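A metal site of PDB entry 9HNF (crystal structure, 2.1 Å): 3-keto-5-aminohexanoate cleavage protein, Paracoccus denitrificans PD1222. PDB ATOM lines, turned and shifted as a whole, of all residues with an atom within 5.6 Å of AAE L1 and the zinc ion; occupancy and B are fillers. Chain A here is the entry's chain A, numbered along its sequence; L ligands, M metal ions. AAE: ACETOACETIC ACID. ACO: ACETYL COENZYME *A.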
ATOM      1  N   ALA A  36       5.107  23.041  27.386  1.00  0.00           N
ATOM      2  CA  ALA A  36       4.677  21.652  27.457  1.00  0.00           C
ATOM      3  C   ALA A  36       4.925  21.153  28.877  1.00  0.00           C
ATOM      4  O   ALA A  36       6.069  20.922  29.262  1.00  0.00           O
ATOM      5  CB  ALA A  36       5.429  20.810  26.425  1.00  0.00           C
ATOM      6  N   GLY A  39       4.080  16.016  29.398  1.00  0.00           N
ATOM      7  CA  GLY A  39       4.422  15.061  28.372  1.00  0.00           C
ATOM      8  C   GLY A  39       4.218  13.605  28.771  1.00  0.00           C
ATOM      9  O   GLY A  39       3.477  13.279  29.712  1.00  0.00           O
ATOM     10  N   HIS A  73       0.842  23.072  25.911  1.00  0.00           N
ATOM     11  CA  HIS A  73       0.773  21.751  25.314  1.00  0.00           C
ATOM     12  C   HIS A  73       0.571  20.730  26.425  1.00  0.00           C
ATOM     13  O   HIS A  73       1.378  20.662  27.365  1.00  0.00           O
ATOM     14  CB  HIS A  73       2.038  21.463  24.518  1.00  0.00           C
ATOM     15  CG  HIS A  73       2.075  20.104  23.893  1.00  0.00           C
ATOM     16  ND1 HIS A  73       1.268  19.757  22.835  1.00  0.00           N
ATOM     17  CD2 HIS A  73       2.823  19.012  24.174  1.00  0.00           C
ATOM     18  CE1 HIS A  73       1.506  18.502  22.487  1.00  0.00           C
ATOM     19  NE2 HIS A  73       2.452  18.037  23.288  1.00  0.00           N
ATOM     20  N   HIS A  75      -0.402  16.895  28.105  1.00  0.00           N
ATOM     21  CA  HIS A  75      -0.624  15.473  28.286  1.00  0.00           C
ATOM     22  C   HIS A  75      -1.287  15.261  29.644  1.00  0.00           C
ATOM     23  O   HIS A  75      -1.294  16.153  30.503  1.00  0.00           O
ATOM     24  CB  HIS A  75       0.676  14.657  28.231  1.00  0.00           C
ATOM     25  CG  HIS A  75       1.329  14.648  26.887  1.00  0.00           C
ATOM     26  ND1 HIS A  75       1.745  13.485  26.278  1.00  0.00           N
ATOM     27  CD2 HIS A  75       1.677  15.661  26.058  1.00  0.00           C
ATOM     28  CE1 HIS A  75       2.311  13.784  25.118  1.00  0.00           C
ATOM     29  NE2 HIS A  75       2.284  15.091  24.960  1.00  0.00           N
ATOM     30  N   THR A 109      -2.287  16.872  22.947  1.00  0.00           N
ATOM     31  CA  THR A 109      -1.453  15.918  22.247  1.00  0.00           C
ATOM     32  C   THR A 109      -2.277  14.883  21.511  1.00  0.00           C
ATOM     33  O   THR A 109      -3.286  14.378  22.026  1.00  0.00           O
ATOM     34  CB  THR A 109      -0.519  15.213  23.243  1.00  0.00           C
ATOM     35  OG1 THR A 109       0.400  14.382  22.516  1.00  0.00           O
ATOM     36  CG2 THR A 109      -1.315  14.340  24.211  1.00  0.00           C
ATOM     37  N   THR A 110      -1.872  14.580  20.279  1.00  0.00           N
ATOM     38  CA  THR A 110      -2.283  13.362  19.595  1.00  0.00           C
ATOM     39  C   THR A 110      -1.141  12.355  19.542  1.00  0.00           C
ATOM     40  O   THR A 110      -1.262  11.323  18.871  1.00  0.00           O
ATOM     41  CB  THR A 110      -2.776  13.645  18.175  1.00  0.00           C
ATOM     42  OG1 THR A 110      -1.652  13.872  17.308  1.00  0.00           O
ATOM     43  CG2 THR A 110      -3.714  14.857  18.137  1.00  0.00           C
ATOM     44  N   GLY A 111      -0.035  12.636  20.215  1.00  0.00           N
ATOM     45  CA  GLY A 111       1.082  11.717  20.255  1.00  0.00           C
ATOM     46  C   GLY A 111       1.023  10.783  21.451  1.00  0.00           C
ATOM     47  O   GLY A 111       1.384   9.614  21.341  1.00  0.00           O
ATOM     48  N   GLY A 112       0.552  11.301  22.588  1.00  0.00           N
ATOM     49  CA  GLY A 112       0.535  10.508  23.800  1.00  0.00           C
ATOM     50  C   GLY A 112       1.891   9.910  24.073  1.00  0.00           C
ATOM     51  O   GLY A 112       2.945  10.514  23.809  1.00  0.00           O
ATOM     52  N   SER A 134      -1.319  18.626  18.462  1.00  0.00           N
ATOM     53  CA  SER A 134      -0.091  18.159  17.829  1.00  0.00           C
ATOM     54  C   SER A 134      -0.410  17.095  16.789  1.00  0.00           C
ATOM     55  O   SER A 134      -1.356  16.318  16.934  1.00  0.00           O
ATOM     56  CB  SER A 134       0.873  17.603  18.875  1.00  0.00           C
ATOM     57  OG  SER A 134       0.381  16.416  19.469  1.00  0.00           O
ATOM     58  N   LEU A 135       0.378  17.083  15.720  1.00  0.00           N
ATOM     59  CA  LEU A 135       0.259  16.092  14.656  1.00  0.00           C
ATOM     60  C   LEU A 135       1.661  15.654  14.283  1.00  0.00           C
ATOM     61  O   LEU A 135       2.410  16.428  13.663  1.00  0.00           O
ATOM     62  CB  LEU A 135      -0.495  16.642  13.444  1.00  0.00           C
ATOM     63  CG  LEU A 135      -0.762  15.650  12.309  1.00  0.00           C
ATOM     64  CD1 LEU A 135      -1.753  14.586  12.745  1.00  0.00           C
ATOM     65  CD2 LEU A 135      -1.260  16.371  11.068  1.00  0.00           C
ATOM     66  N   ASN A 136       2.034  14.437  14.656  1.00  0.00           N
ATOM     67  CA  ASN A 136       3.356  13.930  14.365  1.00  0.00           C
ATOM     68  C   ASN A 136       3.404  13.408  12.935  1.00  0.00           C
ATOM     69  O   ASN A 136       2.511  12.689  12.493  1.00  0.00           O
ATOM     70  CB  ASN A 136       3.731  12.851  15.373  1.00  0.00           C
ATOM     71  CG  ASN A 136       3.685  13.360  16.805  1.00  0.00           C
ATOM     72  OD1 ASN A 136       4.634  13.960  17.294  1.00  0.00           O
ATOM     73  ND2 ASN A 136       2.552  13.142  17.474  1.00  0.00           N
ATOM     74  N   PHE A 171       7.110   4.831  17.005  1.00  0.00           N
ATOM     75  CA  PHE A 171       6.138   5.924  17.083  1.00  0.00           C
ATOM     76  C   PHE A 171       5.456   5.996  15.728  1.00  0.00           C
ATOM     77  O   PHE A 171       6.006   6.540  14.770  1.00  0.00           O
ATOM     78  CB  PHE A 171       6.865   7.225  17.445  1.00  0.00           C
ATOM     79  CG  PHE A 171       5.961   8.384  17.769  1.00  0.00           C
ATOM     80  CD1 PHE A 171       4.660   8.196  18.214  1.00  0.00           C
ATOM     81  CD2 PHE A 171       6.422   9.687  17.624  1.00  0.00           C
ATOM     82  CE1 PHE A 171       3.855   9.273  18.517  1.00  0.00           C
ATOM     83  CE2 PHE A 171       5.614  10.763  17.917  1.00  0.00           C
ATOM     84  CZ  PHE A 171       4.328  10.562  18.358  1.00  0.00           C
ATOM     85  N   GLU A 195       4.496  18.320  14.122  1.00  0.00           N
ATOM     86  CA  GLU A 195       5.736  17.969  14.804  1.00  0.00           C
ATOM     87  C   GLU A 195       6.664  17.265  13.812  1.00  0.00           C
ATOM     88  O   GLU A 195       6.346  16.171  13.330  1.00  0.00           O
ATOM     89  CB  GLU A 195       5.465  17.066  15.997  1.00  0.00           C
ATOM     90  CG  GLU A 195       4.258  17.476  16.828  1.00  0.00           C
ATOM     91  CD  GLU A 195       4.475  18.755  17.605  1.00  0.00           C
ATOM     92  OE1 GLU A 195       5.597  19.313  17.524  1.00  0.00           O
ATOM     93  OE2 GLU A 195       3.540  19.196  18.290  1.00  0.00           O
ATOM     94  N   TYR A 197      10.455  15.808  13.280  1.00  0.00           N
ATOM     95  CA  TYR A 197      11.636  15.351  13.980  1.00  0.00           C
ATOM     96  C   TYR A 197      12.841  15.184  13.053  1.00  0.00           C
ATOM     97  O   TYR A 197      13.929  14.859  13.537  1.00  0.00           O
ATOM     98  CB  TYR A 197      11.347  14.016  14.675  1.00  0.00           C
ATOM     99  CG  TYR A 197      10.210  14.073  15.665  1.00  0.00           C
ATOM    100  CD1 TYR A 197       8.891  14.123  15.233  1.00  0.00           C
ATOM    101  CD2 TYR A 197      10.456  14.063  17.028  1.00  0.00           C
ATOM    102  CE1 TYR A 197       7.850  14.173  16.144  1.00  0.00           C
ATOM    103  CE2 TYR A 197       9.423  14.122  17.946  1.00  0.00           C
ATOM    104  CZ  TYR A 197       8.116  14.172  17.500  1.00  0.00           C
ATOM    105  OH  TYR A 197       7.081  14.216  18.409  1.00  0.00           O
ATOM    106  N   GLN A 221       6.617  22.762  13.949  1.00  0.00           N
ATOM    107  CA  GLN A 221       7.549  22.656  15.066  1.00  0.00           C
ATOM    108  C   GLN A 221       8.615  21.631  14.734  1.00  0.00           C
ATOM    109  O   GLN A 221       8.296  20.451  14.511  1.00  0.00           O
ATOM    110  CB  GLN A 221       6.825  22.275  16.364  1.00  0.00           C
ATOM    111  CG  GLN A 221       7.772  22.218  17.545  1.00  0.00           C
ATOM    112  CD  GLN A 221       7.094  22.640  18.826  1.00  0.00           C
ATOM    113  OE1 GLN A 221       7.277  23.768  19.292  1.00  0.00           O
ATOM    114  NE2 GLN A 221       6.320  21.733  19.414  1.00  0.00           N
ATOM    115  N   VAL A 223      11.700  19.458  15.956  1.00  0.00           N
ATOM    116  CA  VAL A 223      12.077  18.881  17.240  1.00  0.00           C
ATOM    117  C   VAL A 223      13.508  18.357  17.150  1.00  0.00           C
ATOM    118  O   VAL A 223      13.824  17.557  16.263  1.00  0.00           O
ATOM    119  CB  VAL A 223      11.111  17.746  17.634  1.00  0.00           C
ATOM    120  CG1 VAL A 223      11.496  17.160  18.990  1.00  0.00           C
ATOM    121  CG2 VAL A 223       9.677  18.238  17.655  1.00  0.00           C
ATOM    122  N   LEU A 257      11.789  22.961  19.344  1.00  0.00           N
ATOM    123  CA  LEU A 257      11.829  22.241  20.595  1.00  0.00           C
ATOM    124  C   LEU A 257      13.225  21.662  20.740  1.00  0.00           C
ATOM    125  O   LEU A 257      13.639  20.836  19.921  1.00  0.00           O
ATOM    126  CB  LEU A 257      10.773  21.139  20.635  1.00  0.00           C
ATOM    127  CG  LEU A 257      10.552  20.324  21.899  1.00  0.00           C
ATOM    128  CD1 LEU A 257       9.333  19.437  21.695  1.00  0.00           C
ATOM    129  CD2 LEU A 257      11.763  19.480  22.271  1.00  0.00           C
ATOM    130  N   ARG A 278       9.356  26.665  22.254  1.00  0.00           N
ATOM    131  CA  ARG A 278       8.677  25.783  23.188  1.00  0.00           C
ATOM    132  C   ARG A 278       9.633  25.446  24.331  1.00  0.00           C
ATOM    133  O   ARG A 278      10.784  25.085  24.087  1.00  0.00           O
ATOM    134  CB  ARG A 278       8.197  24.499  22.500  1.00  0.00           C
ATOM    135  CG  ARG A 278       7.850  23.373  23.464  1.00  0.00           C
ATOM    136  CD  ARG A 278       7.110  22.236  22.776  1.00  0.00           C
ATOM    137  NE  ARG A 278       7.302  20.974  23.468  1.00  0.00           N
ATOM    138  CZ  ARG A 278       6.564  19.882  23.288  1.00  0.00           C
ATOM    139  NH1 ARG A 278       5.544  19.873  22.449  1.00  0.00           N
ATOM    140  NH2 ARG A 278       6.862  18.781  23.965  1.00  0.00           N
ATOM    141  N   GLU A 282       8.100  18.791  29.965  1.00  0.00           N
ATOM    142  CA  GLU A 282       7.967  17.670  29.033  1.00  0.00           C
ATOM    143  C   GLU A 282       9.276  17.400  28.315  1.00  0.00           C
ATOM    144  O   GLU A 282       9.549  16.261  27.925  1.00  0.00           O
ATOM    145  CB  GLU A 282       6.855  17.946  28.016  1.00  0.00           C
ATOM    146  CG  GLU A 282       6.820  16.978  26.820  1.00  0.00           C
ATOM    147  CD  GLU A 282       5.486  17.000  26.061  1.00  0.00           C
ATOM    148  OE1 GLU A 282       4.542  17.657  26.549  1.00  0.00           O
ATOM    149  OE2 GLU A 282       5.367  16.358  24.995  1.00  0.00           O
ATOM    150  N   ASP A 283      10.111  18.432  28.137  1.00  0.00           N
ATOM    151  CA  ASP A 283      11.299  18.347  27.302  1.00  0.00           C
ATOM    152  C   ASP A 283      12.609  18.487  28.063  1.00  0.00           C
ATOM    153  O   ASP A 283      13.648  18.041  27.568  1.00  0.00           O
ATOM    154  CB  ASP A 283      11.265  19.442  26.223  1.00  0.00           C
ATOM    155  CG  ASP A 283       9.982  19.424  25.421  1.00  0.00           C
ATOM    156  OD1 ASP A 283       9.442  18.326  25.204  1.00  0.00           O
ATOM    157  OD2 ASP A 283       9.517  20.507  25.015  1.00  0.00           O
HETATM  158  O1  AAE L   1       2.823  15.475  22.062  1.00  0.00           O
HETATM  159  C2  AAE L   1       3.087  15.264  20.862  1.00  0.00           C
HETATM  160  O3  AAE L   1       2.261  14.810  20.072  1.00  0.00           O
HETATM  161  C4  AAE L   1       4.461  15.617  20.297  1.00  0.00           C
HETATM  162  C5  AAE L   1       5.395  16.493  21.120  1.00  0.00           C
HETATM  163  O8  AAE L   1       5.170  16.842  22.274  1.00  0.00           O
HETATM  164  C9  AAE L   1       6.640  16.936  20.406  1.00  0.00           C
HETATM  165  N1A ACO L   2      23.906  25.086  32.532  1.00  0.00           N
HETATM  166  C2A ACO L   2      24.761  24.076  32.753  1.00  0.00           C
HETATM  167  N3A ACO L   2      24.517  22.775  32.855  1.00  0.00           N
HETATM  168  C4A ACO L   2      23.210  22.529  32.699  1.00  0.00           C
HETATM  169  C5A ACO L   2      22.212  23.451  32.467  1.00  0.00           C
HETATM  170  C6A ACO L   2      22.594  24.804  32.371  1.00  0.00           C
HETATM  171  N6A ACO L   2      21.757  25.803  32.156  1.00  0.00           N
HETATM  172  N7A ACO L   2      20.984  22.811  32.367  1.00  0.00           N
HETATM  173  C8A ACO L   2      21.255  21.541  32.534  1.00  0.00           C
HETATM  174  N9A ACO L   2      22.596  21.308  32.736  1.00  0.00           N
HETATM  175  C1B ACO L   2      23.263  20.040  32.963  1.00  0.00           C
HETATM  176  C2B ACO L   2      22.887  19.330  34.263  1.00  0.00           C
HETATM  177  O2B ACO L   2      23.573  19.850  35.372  1.00  0.00           O
HETATM  178  C3B ACO L   2      23.303  17.911  33.909  1.00  0.00           C
HETATM  179  O3B ACO L   2      24.718  17.836  33.969  1.00  0.00           O
HETATM  180  P3B ACO L   2      25.267  16.364  34.251  1.00  0.00           P
HETATM  181  O7A ACO L   2      24.984  15.494  33.057  1.00  0.00           O
HETATM  182  O8A ACO L   2      24.630  15.847  35.494  1.00  0.00           O
HETATM  183  O9A ACO L   2      26.736  16.574  34.435  1.00  0.00           O
HETATM  184  C4B ACO L   2      22.812  17.802  32.484  1.00  0.00           C
HETATM  185  O4B ACO L   2      22.902  19.143  31.941  1.00  0.00           O
HETATM  186  C5B ACO L   2      21.394  17.323  32.352  1.00  0.00           C
HETATM  187  O5B ACO L   2      20.845  17.810  31.106  1.00  0.00           O
HETATM  188  P1A ACO L   2      20.787  16.794  29.870  1.00  0.00           P
HETATM  189  O1A ACO L   2      22.177  16.466  29.448  1.00  0.00           O
HETATM  190  O2A ACO L   2      19.847  17.311  28.842  1.00  0.00           O
HETATM  191  O3A ACO L   2      20.144  15.510  30.570  1.00  0.00           O
HETATM  192  P2A ACO L   2      20.207  13.943  30.251  1.00  0.00           P
HETATM  193  O4A ACO L   2      21.562  13.600  29.778  1.00  0.00           O
HETATM  194  O5A ACO L   2      19.645  13.232  31.428  1.00  0.00           O
HETATM  195  O6A ACO L   2      19.199  13.817  29.001  1.00  0.00           O
HETATM  196  CBP ACO L   2      17.049  13.820  27.898  1.00  0.00           C
HETATM  197  CCP ACO L   2      17.811  14.166  29.169  1.00  0.00           C
HETATM  198  CDP ACO L   2      17.482  14.760  26.759  1.00  0.00           C
HETATM  199  CEP ACO L   2      17.376  12.386  27.488  1.00  0.00           C
HETATM  200  CAP ACO L   2      15.551  13.968  28.149  1.00  0.00           C
HETATM  201  OAP ACO L   2      15.359  15.144  28.889  1.00  0.00           O
HETATM  202  C9P ACO L   2      14.725  14.034  26.879  1.00  0.00           C
HETATM  203  O9P ACO L   2      14.686  13.078  26.113  1.00  0.00           O
HETATM  204  N8P ACO L   2      14.083  15.177  26.645  1.00  0.00           N
HETATM  205  C7P ACO L   2      13.042  15.347  25.628  1.00  0.00           C
HETATM  206  C6P ACO L   2      11.859  14.440  25.855  1.00  0.00           C
HETATM  207  C5P ACO L   2      10.969  14.416  24.634  1.00  0.00           C
HETATM  208  O5P ACO L   2      10.938  13.433  23.888  1.00  0.00           O
HETATM  209  N4P ACO L   2      10.179  15.471  24.421  1.00  0.00           N
HETATM  210  C3P ACO L   2       9.516  15.715  23.159  1.00  0.00           C
HETATM  211  C2P ACO L   2       8.057  15.313  23.210  1.00  0.00           C
HETATM  212  S1P ACO L   2       7.574  14.002  22.065  1.00  0.00           S
HETATM  213  C   ACO L   2       5.991  13.369  22.436  1.00  0.00           C
HETATM  214  O   ACO L   2       5.266  13.892  23.229  1.00  0.00           O
HETATM  215  CH3 ACO L   2       5.636  12.145  21.663  1.00  0.00           C
HETATM  216 ZN    ZN M   1       3.793  16.232  23.692  1.00  0.00          ZN
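O1 of AAE L1 is bound to the zinc ion, at 2.0 Å.
The zinc ion is bound by the side-chain carboxylate (OE2) of Glu 282, at 2.0 Å.
O8 of AAE L1 is bound to the zinc ion (2.1 Å).
The zinc ion is bound by NE2 of His 75 (2.3 Å).
NE2 of His 73 binds the zinc ion, 2.3 Å away.
The zinc ion has five donor atoms within binding distance.
Slightly farther from the zinc ion lies an oxygen (O) of ACO L2 (2.8 Å).
The side-chain carboxylate (OE1) of Glu 282 is in salt-bridge range of the guanidinium group (NH2) of Arg 278 (3.7 Å).
The backbone NH (N) of Gly 39 sits close to the side-chain carboxylate (OE1) of Glu 282 (3.3 Å).
The backbone NH of Glu 282 is in hydrogen-bond range of the backbone carbonyl oxygen of Ala 36 (3.0 Å).
The side-chain hydroxyl of Thr 110 lies within hydrogen-bond range of the backbone carbonyl oxygen of Ser 134 (2.5 Å).
The side-chain carboxylate (OD2) of Asp 283 lies within salt-bridge range of the guanidinium group (NE) of Arg 278 (2.7 Å).
OH of Tyr 197 is in hydrogen-bond range of OD1 of Asn 136 (2.7 Å).
OE1 of Glu 195 sits at hydrogen-bond distance from NE2 of Gln 221 (3.2 Å).
N of Glu 195 sits at hydrogen-bond distance from O of Leu 135 (2.9 Å).
O3 of AAE L1 lies within hydrogen-bond range of OG of Ser 134 (2.5 Å).
O3 of AAE L1 lies within hydrogen-bond range of OG1 of Thr 109 (3.1 Å).
O8 of AAE L1 lies close to NH1 of Arg 278 (3.1 Å).
The side-chain amide nitrogen (ND2) of Asn 136 is in hydrogen-bond range of an oxygen (O3) of AAE L1 (3.1 Å).
An oxygen (O3) of AAE L1 sits at hydrogen-bond distance from the backbone NH of Gly 111 (3.2 Å).
A sulfur (S1P) of ACO L2 lies close to the side-chain hydroxyl of Tyr 197 (3.7 Å).
O of Asp 283 lies within hydrogen-bond range of N8P of ACO L2 (3.0 Å).
OD1 of Asp 283 lies within hydrogen-bond range of N4P of ACO L2 (3.1 Å).
OE1 of Glu 195 touches C9 of AAE L1, 3.9 Å away.
Tyr 197 touches AAE L1 (OH to C9, 3.4 Å).
Leu 257 touches AAE L1.
Hydrophobic or aromatic side chains that line AAE L1: His 73, His 75 and Leu 257.
Within 4 Å of AAE L1: His 73, His 75, Thr 109, Gly 111, Ser 134, Asn 136, Glu 195, Tyr 197, Leu 257, Arg 278 and Glu 282.
The nearest printed residue that does not touch AAE L1 is Thr 110 (4.1 Å).
Residues that only touch the zinc ion: Arg 278 (3.999 Å).
Four residues have an atom within 4 Å of the zinc ion: His 73, His 75, Arg 278 and Glu 282.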
